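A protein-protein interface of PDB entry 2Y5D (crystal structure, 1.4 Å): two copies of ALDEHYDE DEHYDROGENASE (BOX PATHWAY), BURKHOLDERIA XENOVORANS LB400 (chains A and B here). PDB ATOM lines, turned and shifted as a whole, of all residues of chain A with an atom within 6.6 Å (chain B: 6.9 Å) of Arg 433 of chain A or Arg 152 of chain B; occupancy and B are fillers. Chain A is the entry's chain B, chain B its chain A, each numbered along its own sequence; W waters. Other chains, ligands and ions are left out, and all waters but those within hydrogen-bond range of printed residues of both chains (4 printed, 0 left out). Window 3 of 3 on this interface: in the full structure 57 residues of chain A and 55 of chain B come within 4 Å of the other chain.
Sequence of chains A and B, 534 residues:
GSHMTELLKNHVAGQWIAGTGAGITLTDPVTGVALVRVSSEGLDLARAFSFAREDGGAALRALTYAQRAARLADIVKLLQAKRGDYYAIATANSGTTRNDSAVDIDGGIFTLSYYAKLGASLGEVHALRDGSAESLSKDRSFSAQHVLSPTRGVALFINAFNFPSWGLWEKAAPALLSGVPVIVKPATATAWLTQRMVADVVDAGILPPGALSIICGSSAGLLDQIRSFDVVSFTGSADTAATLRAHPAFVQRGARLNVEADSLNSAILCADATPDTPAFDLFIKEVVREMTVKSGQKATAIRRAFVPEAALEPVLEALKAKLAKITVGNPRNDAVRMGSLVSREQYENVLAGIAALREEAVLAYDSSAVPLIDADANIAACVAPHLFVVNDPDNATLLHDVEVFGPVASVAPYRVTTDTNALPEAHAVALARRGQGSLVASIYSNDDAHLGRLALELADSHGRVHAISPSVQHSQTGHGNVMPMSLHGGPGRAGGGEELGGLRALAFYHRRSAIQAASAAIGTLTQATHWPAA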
ATOM      1  N   SER A 266       6.233  26.315  30.269  1.00  0.00           N
ATOM      2  CA  SER A 266       6.470  24.883  29.891  1.00  0.00           C
ATOM      3  C   SER A 266       7.424  24.776  28.721  1.00  0.00           C
ATOM      4  O   SER A 266       7.528  25.624  27.854  1.00  0.00           O
ATOM      5  CB  SER A 266       5.176  24.301  29.442  1.00  0.00           C
ATOM      6  OG  SER A 266       4.156  24.286  30.476  1.00  0.00           O
ATOM      7  N   ARG A 304       8.428  23.943  34.007  1.00  0.00           N
ATOM      8  CA  ARG A 304       7.805  22.622  33.847  1.00  0.00           C
ATOM      9  C   ARG A 304       8.236  22.103  32.513  1.00  0.00           C
ATOM     10  O   ARG A 304       7.975  22.697  31.479  1.00  0.00           O
ATOM     11  CB  ARG A 304       6.271  22.742  33.957  1.00  0.00           C
ATOM     12  CG  ARG A 304       5.766  23.258  35.299  1.00  0.00           C
ATOM     13  CD  ARG A 304       4.236  23.341  35.345  1.00  0.00           C
ATOM     14  NE  ARG A 304       3.728  24.318  34.311  1.00  0.00           N
ATOM     15  CZ  ARG A 304       2.589  24.203  33.666  1.00  0.00           C
ATOM     16  NH1 ARG A 304       1.697  23.187  33.898  1.00  0.00           N
ATOM     17  NH2 ARG A 304       2.327  25.141  32.754  1.00  0.00           N
ATOM     18  N   PHE A 306       7.784  18.834  30.062  1.00  0.00           N
ATOM     19  CA  PHE A 306       6.922  17.629  29.884  1.00  0.00           C
ATOM     20  C   PHE A 306       7.482  16.817  28.737  1.00  0.00           C
ATOM     21  O   PHE A 306       7.702  17.313  27.637  1.00  0.00           O
ATOM     22  CB  PHE A 306       5.519  18.137  29.496  1.00  0.00           C
ATOM     23  CG  PHE A 306       4.828  18.840  30.612  1.00  0.00           C
ATOM     24  CD1 PHE A 306       4.482  18.203  31.768  1.00  0.00           C
ATOM     25  CD2 PHE A 306       4.560  20.230  30.489  1.00  0.00           C
ATOM     26  CE1 PHE A 306       3.856  18.935  32.787  1.00  0.00           C
ATOM     27  CE2 PHE A 306       3.916  20.913  31.490  1.00  0.00           C
ATOM     28  CZ  PHE A 306       3.591  20.285  32.688  1.00  0.00           C
ATOM     29  N   ALA A 426      -1.090  15.841  22.866  1.00  0.00           N
ATOM     30  CA  ALA A 426      -2.312  16.386  23.466  1.00  0.00           C
ATOM     31  C   ALA A 426      -2.304  16.445  24.989  1.00  0.00           C
ATOM     32  O   ALA A 426      -2.733  17.454  25.584  1.00  0.00           O
ATOM     33  CB  ALA A 426      -3.576  15.611  22.977  1.00  0.00           C
ATOM     34  N   ALA A 428       0.402  16.703  26.956  1.00  0.00           N
ATOM     35  CA  ALA A 428       1.329  17.787  27.311  1.00  0.00           C
ATOM     36  C   ALA A 428       0.619  19.125  27.166  1.00  0.00           C
ATOM     37  O   ALA A 428       0.931  19.977  28.011  1.00  0.00           O
ATOM     38  CB  ALA A 428       2.501  17.696  26.430  1.00  0.00           C
ATOM     39  N   VAL A 429      -0.224  19.332  26.176  1.00  0.00           N
ATOM     40  CA  VAL A 429      -0.911  20.652  25.959  1.00  0.00           C
ATOM     41  C   VAL A 429      -1.853  20.802  27.149  1.00  0.00           C
ATOM     42  O   VAL A 429      -1.889  21.905  27.704  1.00  0.00           O
ATOM     43  CB  VAL A 429      -1.639  20.649  24.636  1.00  0.00           C
ATOM     44  CG1 VAL A 429      -2.548  21.900  24.468  1.00  0.00           C
ATOM     45  CG2 VAL A 429      -0.687  20.605  23.420  1.00  0.00           C
ATOM     46  N   ALA A 430      -2.613  19.771  27.562  1.00  0.00           N
ATOM     47  CA  ALA A 430      -3.526  19.888  28.646  1.00  0.00           C
ATOM     48  C   ALA A 430      -2.720  20.200  29.916  1.00  0.00           C
ATOM     49  O   ALA A 430      -3.139  21.053  30.739  1.00  0.00           O
ATOM     50  CB  ALA A 430      -4.326  18.569  28.770  1.00  0.00           C
ATOM     51  N   LEU A 431      -1.588  19.537  30.117  1.00  0.00           N
ATOM     52  CA  LEU A 431      -0.760  19.785  31.261  1.00  0.00           C
ATOM     53  C   LEU A 431      -0.250  21.241  31.288  1.00  0.00           C
ATOM     54  O   LEU A 431      -0.271  21.899  32.292  1.00  0.00           O
ATOM     55  CB  LEU A 431       0.427  18.803  31.325  1.00  0.00           C
ATOM     56  CG  LEU A 431      -0.072  17.397  31.769  1.00  0.00           C
ATOM     57  CD1 LEU A 431       1.095  16.387  31.595  1.00  0.00           C
ATOM     58  CD2 LEU A 431      -0.620  17.258  33.120  1.00  0.00           C
ATOM     59  N   ALA A 432       0.250  21.694  30.165  1.00  0.00           N
ATOM     60  CA  ALA A 432       0.676  23.089  30.099  1.00  0.00           C
ATOM     61  C   ALA A 432      -0.428  24.017  30.495  1.00  0.00           C
ATOM     62  O   ALA A 432      -0.144  24.999  31.200  1.00  0.00           O
ATOM     63  CB  ALA A 432       1.190  23.433  28.702  1.00  0.00           C
ATOM     64  N   ARG A 433      -1.667  23.794  30.032  1.00  0.00           N
ATOM     65  CA  ARG A 433      -2.770  24.656  30.357  1.00  0.00           C
ATOM     66  C   ARG A 433      -3.024  24.672  31.875  1.00  0.00           C
ATOM     67  O   ARG A 433      -3.528  25.677  32.374  1.00  0.00           O
ATOM     68  CB  ARG A 433      -4.009  24.152  29.631  1.00  0.00           C
ATOM     69  CG  ARG A 433      -5.221  25.122  29.431  1.00  0.00           C
ATOM     70  CD  ARG A 433      -6.134  24.341  28.318  1.00  0.00           C
ATOM     71  NE  ARG A 433      -5.592  24.316  26.954  1.00  0.00           N
ATOM     72  CZ  ARG A 433      -5.882  23.370  26.070  1.00  0.00           C
ATOM     73  NH1 ARG A 433      -6.596  22.334  26.515  1.00  0.00           N
ATOM     74  NH2 ARG A 433      -5.462  23.412  24.794  1.00  0.00           N
ATOM     75  N   ARG A 434      -2.653  23.615  32.611  1.00  0.00           N
ATOM     76  CA  ARG A 434      -2.910  23.584  34.072  1.00  0.00           C
ATOM     77  C   ARG A 434      -2.068  24.626  34.793  1.00  0.00           C
ATOM     78  O   ARG A 434      -2.332  24.907  35.925  1.00  0.00           O
ATOM     79  CB  ARG A 434      -2.589  22.153  34.640  1.00  0.00           C
ATOM     80  CG  ARG A 434      -3.482  21.160  34.082  1.00  0.00           C
ATOM     81  CD  ARG A 434      -4.419  20.482  34.994  1.00  0.00           C
ATOM     82  NE  ARG A 434      -4.253  20.567  36.450  1.00  0.00           N
ATOM     83  CZ  ARG A 434      -3.965  19.498  37.205  1.00  0.00           C
ATOM     84  NH1 ARG A 434      -3.904  18.296  36.659  1.00  0.00           N
ATOM     85  NH2 ARG A 434      -3.852  19.647  38.519  1.00  0.00           N
ATOM     86  N   GLY A 435      -1.087  25.245  34.105  1.00  0.00           N
ATOM     87  CA  GLY A 435      -0.359  26.404  34.686  1.00  0.00           C
ATOM     88  C   GLY A 435      -1.221  27.698  34.759  1.00  0.00           C
ATOM     89  O   GLY A 435      -0.782  28.634  35.356  1.00  0.00           O
ATOM     90  N   GLN A 436      -2.424  27.599  34.236  1.00  0.00           N
ATOM     91  CA  GLN A 436      -3.472  28.704  34.402  1.00  0.00           C
ATOM     92  C   GLN A 436      -3.121  29.946  33.663  1.00  0.00           C
ATOM     93  O   GLN A 436      -3.596  31.043  33.950  1.00  0.00           O
ATOM     94  CB  GLN A 436      -3.665  29.044  35.907  1.00  0.00           C
ATOM     95  CG  GLN A 436      -3.936  27.802  36.784  1.00  0.00           C
ATOM     96  CD  GLN A 436      -5.265  27.570  36.991  1.00  0.00           C
ATOM     97  OE1 GLN A 436      -6.068  27.591  36.047  1.00  0.00           O
ATOM     98  NE2 GLN A 436      -5.601  27.329  38.259  1.00  0.00           N
ATOM     99  N   GLY A 437      -2.292  29.769  32.607  1.00  0.00           N
ATOM    100  CA  GLY A 437      -1.944  30.901  31.688  1.00  0.00           C
ATOM    101  C   GLY A 437      -0.511  31.355  31.934  1.00  0.00           C
ATOM    102  O   GLY A 437      -0.126  31.712  33.067  1.00  0.00           O
ATOM    103  N   GLU A 457      -2.353  24.900  19.242  1.00  0.00           N
ATOM    104  CA  GLU A 457      -3.049  24.370  20.297  1.00  0.00           C
ATOM    105  C   GLU A 457      -2.640  24.972  21.669  1.00  0.00           C
ATOM    106  O   GLU A 457      -3.379  24.848  22.682  1.00  0.00           O
ATOM    107  CB  GLU A 457      -2.776  22.821  20.301  1.00  0.00           C
ATOM    108  CG  GLU A 457      -3.717  22.087  19.304  1.00  0.00           C
ATOM    109  CD  GLU A 457      -5.169  22.103  19.818  1.00  0.00           C
ATOM    110  OE1 GLU A 457      -5.496  21.568  20.919  1.00  0.00           O
ATOM    111  OE2 GLU A 457      -6.019  22.780  19.172  1.00  0.00           O
ATOM    112  N   LEU A 458      -1.449  25.578  21.737  1.00  0.00           N
ATOM    113  CA  LEU A 458      -0.958  26.218  22.998  1.00  0.00           C
ATOM    114  C   LEU A 458      -1.318  27.700  22.985  1.00  0.00           C
ATOM    115  O   LEU A 458      -1.176  28.329  24.029  1.00  0.00           O
ATOM    116  CB  LEU A 458       0.597  26.076  23.020  1.00  0.00           C
ATOM    117  CG  LEU A 458       0.990  24.597  23.298  1.00  0.00           C
ATOM    118  CD1 LEU A 458       2.360  24.401  22.777  1.00  0.00           C
ATOM    119  CD2 LEU A 458       0.895  24.332  24.840  1.00  0.00           C
ATOM    120  N   ASP A 460      -3.854  29.757  22.895  1.00  0.00           N
ATOM    121  CA  ASP A 460      -4.820  30.471  23.695  1.00  0.00           C
ATOM    122  C   ASP A 460      -4.490  30.540  25.188  1.00  0.00           C
ATOM    123  O   ASP A 460      -5.196  31.231  25.889  1.00  0.00           O
ATOM    124  CB  ASP A 460      -6.257  29.887  23.442  1.00  0.00           C
ATOM    125  CG  ASP A 460      -6.480  28.538  24.009  1.00  0.00           C
ATOM    126  OD1 ASP A 460      -5.802  28.059  24.942  1.00  0.00           O
ATOM    127  OD2 ASP A 460      -7.425  27.799  23.427  1.00  0.00           O
ATOM    128  N   SER A 461      -3.415  29.845  25.602  1.00  0.00           N
ATOM    129  CA  SER A 461      -3.078  29.864  26.983  1.00  0.00           C
ATOM    130  C   SER A 461      -1.653  30.451  27.236  1.00  0.00           C
ATOM    131  O   SER A 461      -1.165  30.468  28.390  1.00  0.00           O
ATOM    132  CB  SER A 461      -3.233  28.507  27.570  1.00  0.00           C
ATOM    133  OG  SER A 461      -2.403  27.558  26.927  1.00  0.00           O
ATOM    134  N   HIS A 462      -0.946  30.775  26.157  1.00  0.00           N
ATOM    135  CA  HIS A 462       0.468  31.259  26.241  1.00  0.00           C
ATOM    136  C   HIS A 462       0.567  32.501  25.410  1.00  0.00           C
ATOM    137  O   HIS A 462       0.245  32.450  24.182  1.00  0.00           O
ATOM    138  CB  HIS A 462       1.470  30.167  25.733  1.00  0.00           C
ATOM    139  CG  HIS A 462       1.407  28.939  26.599  1.00  0.00           C
ATOM    140  ND1 HIS A 462       0.403  27.972  26.494  1.00  0.00           N
ATOM    141  CD2 HIS A 462       2.203  28.544  27.623  1.00  0.00           C
ATOM    142  CE1 HIS A 462       0.574  27.064  27.468  1.00  0.00           C
ATOM    143  NE2 HIS A 462       1.665  27.369  28.158  1.00  0.00           N
ATOM    144  N   ARG B  53     -19.457  27.770  29.375  1.00  0.00           N
ATOM    145  CA  ARG B  53     -17.939  27.787  29.166  1.00  0.00           C
ATOM    146  C   ARG B  53     -17.466  26.535  28.438  1.00  0.00           C
ATOM    147  O   ARG B  53     -16.665  26.589  27.497  1.00  0.00           O
ATOM    148  CB  ARG B  53     -17.240  28.094  30.454  1.00  0.00           C
ATOM    149  CG  ARG B  53     -15.802  28.526  30.157  1.00  0.00           C
ATOM    150  CD  ARG B  53     -15.057  28.873  31.360  1.00  0.00           C
ATOM    151  NE  ARG B  53     -15.667  29.968  32.131  1.00  0.00           N
ATOM    152  CZ  ARG B  53     -16.351  29.843  33.285  1.00  0.00           C
ATOM    153  NH1 ARG B  53     -16.626  28.568  33.814  1.00  0.00           N
ATOM    154  NH2 ARG B  53     -16.822  30.912  33.924  1.00  0.00           N
ATOM    155  N   GLU B  54     -17.955  25.389  28.931  1.00  0.00           N
ATOM    156  CA  GLU B  54     -17.448  24.105  28.394  1.00  0.00           C
ATOM    157  C   GLU B  54     -18.178  23.638  27.187  1.00  0.00           C
ATOM    158  O   GLU B  54     -17.627  23.574  26.088  1.00  0.00           O
ATOM    159  CB  GLU B  54     -17.491  23.043  29.475  1.00  0.00           C
ATOM    160  CG  GLU B  54     -17.133  23.413  30.847  1.00  0.00           C
ATOM    161  CD  GLU B  54     -15.778  23.440  31.230  1.00  0.00           C
ATOM    162  OE1 GLU B  54     -14.888  24.210  30.678  1.00  0.00           O
ATOM    163  OE2 GLU B  54     -15.617  22.672  32.218  1.00  0.00           O
ATOM    164  N   GLY B  57     -18.641  26.827  24.650  1.00  0.00           N
ATOM    165  CA  GLY B  57     -17.415  27.213  23.956  1.00  0.00           C
ATOM    166  C   GLY B  57     -16.817  26.138  23.078  1.00  0.00           C
ATOM    167  O   GLY B  57     -16.282  26.415  22.001  1.00  0.00           O
ATOM    168  N   ARG B  61     -16.152  26.848  19.173  1.00  0.00           N
ATOM    169  CA  ARG B  61     -14.782  26.777  18.662  1.00  0.00           C
ATOM    170  C   ARG B  61     -14.569  25.713  17.656  1.00  0.00           C
ATOM    171  O   ARG B  61     -13.649  25.821  16.795  1.00  0.00           O
ATOM    172  CB  ARG B  61     -13.751  26.562  19.733  1.00  0.00           C
ATOM    173  CG  ARG B  61     -13.578  27.901  20.601  1.00  0.00           C
ATOM    174  CD  ARG B  61     -12.449  27.718  21.603  1.00  0.00           C
ATOM    175  NE  ARG B  61     -12.484  26.489  22.452  1.00  0.00           N
ATOM    176  CZ  ARG B  61     -13.080  26.487  23.608  1.00  0.00           C
ATOM    177  NH1 ARG B  61     -13.749  27.518  24.094  1.00  0.00           N
ATOM    178  NH2 ARG B  61     -13.118  25.357  24.287  1.00  0.00           N
ATOM    179  N   SER B 149      -6.538  33.757  18.980  1.00  0.00           N
ATOM    180  CA  SER B 149      -7.302  32.498  19.194  1.00  0.00           C
ATOM    181  C   SER B 149      -8.473  32.792  20.176  1.00  0.00           C
ATOM    182  O   SER B 149      -8.265  33.592  21.113  1.00  0.00           O
ATOM    183  CB  SER B 149      -6.405  31.451  19.934  1.00  0.00           C
ATOM    184  OG  SER B 149      -5.215  31.229  19.222  1.00  0.00           O
ATOM    185  N   PRO B 150      -9.627  32.223  19.980  1.00  0.00           N
ATOM    186  CA  PRO B 150     -10.764  32.526  20.815  1.00  0.00           C
ATOM    187  C   PRO B 150     -10.397  32.236  22.275  1.00  0.00           C
ATOM    188  O   PRO B 150      -9.814  31.180  22.641  1.00  0.00           O
ATOM    189  CB  PRO B 150     -11.858  31.513  20.300  1.00  0.00           C
ATOM    190  CG  PRO B 150     -11.531  31.363  18.818  1.00  0.00           C
ATOM    191  CD  PRO B 150      -9.994  31.315  18.815  1.00  0.00           C
ATOM    192  N   THR B 151     -10.811  33.137  23.179  1.00  0.00           N
ATOM    193  CA  THR B 151     -10.616  32.861  24.622  1.00  0.00           C
ATOM    194  C   THR B 151     -11.490  31.670  25.080  1.00  0.00           C
ATOM    195  O   THR B 151     -12.665  31.551  24.720  1.00  0.00           O
ATOM    196  CB  THR B 151     -10.817  34.137  25.487  1.00  0.00           C
ATOM    197  OG1 THR B 151     -10.311  33.875  26.800  1.00  0.00           O
ATOM    198  CG2 THR B 151     -12.321  34.595  25.495  1.00  0.00           C
ATOM    199  N   ARG B 152     -10.880  30.831  25.905  1.00  0.00           N
ATOM    200  CA  ARG B 152     -11.669  29.705  26.500  1.00  0.00           C
ATOM    201  C   ARG B 152     -12.449  30.105  27.732  1.00  0.00           C
ATOM    202  O   ARG B 152     -12.144  29.780  28.936  1.00  0.00           O
ATOM    203  CB  ARG B 152     -10.657  28.574  26.841  1.00  0.00           C
ATOM    204  CG  ARG B 152     -10.184  27.881  25.619  1.00  0.00           C
ATOM    205  CD  ARG B 152      -9.188  26.716  26.106  1.00  0.00           C
ATOM    206  NE  ARG B 152      -8.822  25.922  24.946  1.00  0.00           N
ATOM    207  CZ  ARG B 152      -9.129  24.658  24.769  1.00  0.00           C
ATOM    208  NH1 ARG B 152      -9.818  23.995  25.683  1.00  0.00           N
ATOM    209  NH2 ARG B 152      -8.753  24.104  23.627  1.00  0.00           N
ATOM    210  N   GLY B 153     -13.381  31.024  27.506  1.00  0.00           N
ATOM    211  CA  GLY B 153     -14.223  31.615  28.527  1.00  0.00           C
ATOM    212  C   GLY B 153     -15.610  31.866  27.973  1.00  0.00           C
ATOM    213  O   GLY B 153     -15.977  31.393  26.890  1.00  0.00           O
ATOM    214  N   VAL B 154     -16.327  32.607  28.789  1.00  0.00           N
ATOM    215  CA  VAL B 154     -17.681  33.100  28.426  1.00  0.00           C
ATOM    216  C   VAL B 154     -17.593  34.628  28.377  1.00  0.00           C
ATOM    217  O   VAL B 154     -16.677  35.223  28.988  1.00  0.00           O
ATOM    218  CB  VAL B 154     -18.745  32.692  29.392  1.00  0.00           C
ATOM    219  CG1 VAL B 154     -18.767  31.180  29.586  1.00  0.00           C
ATOM    220  CG2 VAL B 154     -18.556  33.375  30.744  1.00  0.00           C
ATOM    221  N   VAL B 180     -17.035  32.760  21.173  1.00  0.00           N
ATOM    222  CA  VAL B 180     -17.100  32.873  22.630  1.00  0.00           C
ATOM    223  C   VAL B 180     -18.578  32.836  22.967  1.00  0.00           C
ATOM    224  O   VAL B 180     -19.370  33.613  22.431  1.00  0.00           O
ATOM    225  CB  VAL B 180     -16.417  34.180  23.125  1.00  0.00           C
ATOM    226  CG1 VAL B 180     -16.567  34.297  24.566  1.00  0.00           C
ATOM    227  CG2 VAL B 180     -14.907  34.132  22.759  1.00  0.00           C
ATOM    228  N   PRO B 181     -18.964  31.907  23.876  1.00  0.00           N
ATOM    229  CA  PRO B 181     -20.404  31.842  24.256  1.00  0.00           C
ATOM    230  C   PRO B 181     -20.865  33.066  25.084  1.00  0.00           C
ATOM    231  O   PRO B 181     -20.049  33.670  25.825  1.00  0.00           O
ATOM    232  CB  PRO B 181     -20.484  30.552  25.100  1.00  0.00           C
ATOM    233  CG  PRO B 181     -19.093  30.268  25.528  1.00  0.00           C
ATOM    234  CD  PRO B 181     -18.096  30.905  24.516  1.00  0.00           C
ATOM    235  N   SER B 228     -10.789  33.541  34.951  1.00  0.00           N
ATOM    236  CA  SER B 228      -9.726  34.363  34.403  1.00  0.00           C
ATOM    237  C   SER B 228      -9.706  34.487  32.876  1.00  0.00           C
ATOM    238  O   SER B 228      -9.102  35.470  32.351  1.00  0.00           O
ATOM    239  CB  SER B 228      -8.339  33.852  34.906  1.00  0.00           C
ATOM    240  OG  SER B 228      -8.295  32.503  34.370  1.00  0.00           O
ATOM    241  N   PHE B 229     -10.369  33.598  32.139  1.00  0.00           N
ATOM    242  CA  PHE B 229     -10.408  33.669  30.648  1.00  0.00           C
ATOM    243  C   PHE B 229     -11.706  34.222  30.131  1.00  0.00           C
ATOM    244  O   PHE B 229     -11.936  34.196  28.894  1.00  0.00           O
ATOM    245  CB  PHE B 229     -10.029  32.316  30.006  1.00  0.00           C
ATOM    246  CG  PHE B 229      -8.739  31.821  30.506  1.00  0.00           C
ATOM    247  CD1 PHE B 229      -7.536  32.371  30.131  1.00  0.00           C
ATOM    248  CD2 PHE B 229      -8.714  30.782  31.388  1.00  0.00           C
ATOM    249  CE1 PHE B 229      -6.225  31.770  30.625  1.00  0.00           C
ATOM    250  CE2 PHE B 229      -7.488  30.228  31.883  1.00  0.00           C
ATOM    251  CZ  PHE B 229      -6.268  30.775  31.525  1.00  0.00           C
ATOM    252  N   ASP B 230     -12.588  34.599  31.074  1.00  0.00           N
ATOM    253  CA  ASP B 230     -13.882  35.206  30.695  1.00  0.00           C
ATOM    254  C   ASP B 230     -13.693  36.669  30.397  1.00  0.00           C
ATOM    255  O   ASP B 230     -12.695  37.333  30.741  1.00  0.00           O
ATOM    256  CB  ASP B 230     -14.802  35.006  31.900  1.00  0.00           C
ATOM    257  CG  ASP B 230     -15.179  33.559  32.135  1.00  0.00           C
ATOM    258  OD1 ASP B 230     -14.955  32.667  31.293  1.00  0.00           O
ATOM    259  OD2 ASP B 230     -15.716  33.404  33.236  1.00  0.00           O
ATOM    260  N   TYR B 509     -12.332  39.461  22.417  1.00  0.00           N
ATOM    261  CA  TYR B 509     -12.746  38.046  22.513  1.00  0.00           C
ATOM    262  C   TYR B 509     -11.669  37.034  22.301  1.00  0.00           C
ATOM    263  O   TYR B 509     -11.901  35.816  22.417  1.00  0.00           O
ATOM    264  CB  TYR B 509     -13.948  37.768  21.679  1.00  0.00           C
ATOM    265  CG  TYR B 509     -15.085  38.670  22.051  1.00  0.00           C
ATOM    266  CD1 TYR B 509     -15.835  38.377  23.207  1.00  0.00           C
ATOM    267  CD2 TYR B 509     -15.435  39.820  21.316  1.00  0.00           C
ATOM    268  CE1 TYR B 509     -16.895  39.236  23.618  1.00  0.00           C
ATOM    269  CE2 TYR B 509     -16.443  40.647  21.690  1.00  0.00           C
ATOM    270  CZ  TYR B 509     -17.148  40.363  22.830  1.00  0.00           C
ATOM    271  OH  TYR B 509     -18.164  41.206  23.249  1.00  0.00           O
ATOM    272  N   ARG B 511      -7.268  35.795  22.504  1.00  0.00           N
ATOM    273  CA  ARG B 511      -5.975  35.856  23.099  1.00  0.00           C
ATOM    274  C   ARG B 511      -4.952  35.968  21.945  1.00  0.00           C
ATOM    275  O   ARG B 511      -5.012  35.139  21.016  1.00  0.00           O
ATOM    276  CB  ARG B 511      -5.777  34.467  23.833  1.00  0.00           C
ATOM    277  CG  ARG B 511      -7.005  34.050  24.682  1.00  0.00           C
ATOM    278  CD  ARG B 511      -6.848  34.210  26.176  1.00  0.00           C
ATOM    279  NE  ARG B 511      -6.573  35.566  26.683  1.00  0.00           N
ATOM    280  CZ  ARG B 511      -7.331  36.168  27.629  1.00  0.00           C
ATOM    281  NH1 ARG B 511      -8.615  35.849  27.870  1.00  0.00           N
ATOM    282  NH2 ARG B 511      -6.861  37.283  28.179  1.00  0.00           N
HETATM  283  O   HOH W   1      -6.785  25.454  21.555  1.00  0.00           O
HETATM  284  O   HOH W   2      -8.032  30.799  26.644  1.00  0.00           O
HETATM  285  O   HOH W   3      -8.960  28.859  21.575  1.00  0.00           O
HETATM  286  O   HOH W   4      -5.821  31.777  35.394  1.00  0.00           O
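O of Ser 149 of chain B lies within hydrogen-bond range of N of Arg 511 of chain B. The side-chain hydroxyl (OG1) of Thr 151 of chain B lies within hydrogen-bond range of the backbone carbonyl oxygen (O) of Phe 229 of chain B (2.7 Å). The side-chain hydroxyl of Thr 151 of chain B lies within hydrogen-bond range of the guanidinium group of Arg 511 of chain B (2.8 Å). The guanidinium group (NH2) of Arg 433 of chain A is in hydrogen-bond range of the backbone carbonyl oxygen (O) of Glu 457 of chain A, 3.3 Å away.
No position is printed for both chains.
The guanidinium group (NE) of Arg 152 of chain B is in salt-bridge range of the side-chain carboxylate (OD2) of Asp 460 of chain A (2.8 Å).
Among the printed residues, pairs that only touch across the chains: Arg 433 of chain A with Arg 152 of chain B, Gln 436 of chain A with Phe 229 of chain B, Asp 460 of chain A with Ser 149 of chain B, Asp 460 of chain A with Pro 150 of chain B and Asp 460 of chain A with Arg 511 of chain B.
Water W3 bridges the side-chain carboxylate (OD2) of Asp 460 of chain A (2.6 Å) and the backbone carbonyl oxygen (O) of Pro 150 of chain B (2.7 Å). Water W4 lies within hydrogen-bond range of O of Gln 436 of chain A (2.8 Å) and OG of Ser 228 of chain B (2.8 Å). Water W2 lies within hydrogen-bond range of N of Arg 152 of chain B (2.9 Å) and O of Asp 460 of chain A (3.0 Å). Water W1 bridges OD2 of Asp 460 of chain A (3.1 Å) and NH2 of Arg 152 of chain B (3.2 Å).
Hydrophobic or aromatic side chains of chain B within 4 Å of the printed part of chain A: Phe 229. Of the 19 printed residues of chain A, 3 touch a printed residue of chain B. Among the printed residues, Asp or Glu carboxylates within 4 Å of a Lys or Arg side-chain nitrogen of the other chain: Asp 460 of chain A with Arg 152 of chain B.
Of chain B, only Arg 152 comes within 4 Å of Arg 433 of chain A. Arg 152 of chain B touches two residues of chain A. Printed residues of chain B within 4 Å of Gln 436 of chain A: Phe 229. Printed residues of chain A within 4 Å of Pro 150 of chain B: Asp 460. Ala 430 of chain A touches none of the printed residues of chain B. Arg 434 of chain A touches none of the printed residues of chain B. The nearest residue of chain B that does not touch Arg 433 of chain A is Phe 229 of chain B (5.8 Å). The nearest printed residue of chain A that does not touch Arg 511 of chain B is Ser 461 of chain A (5.5 Å).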
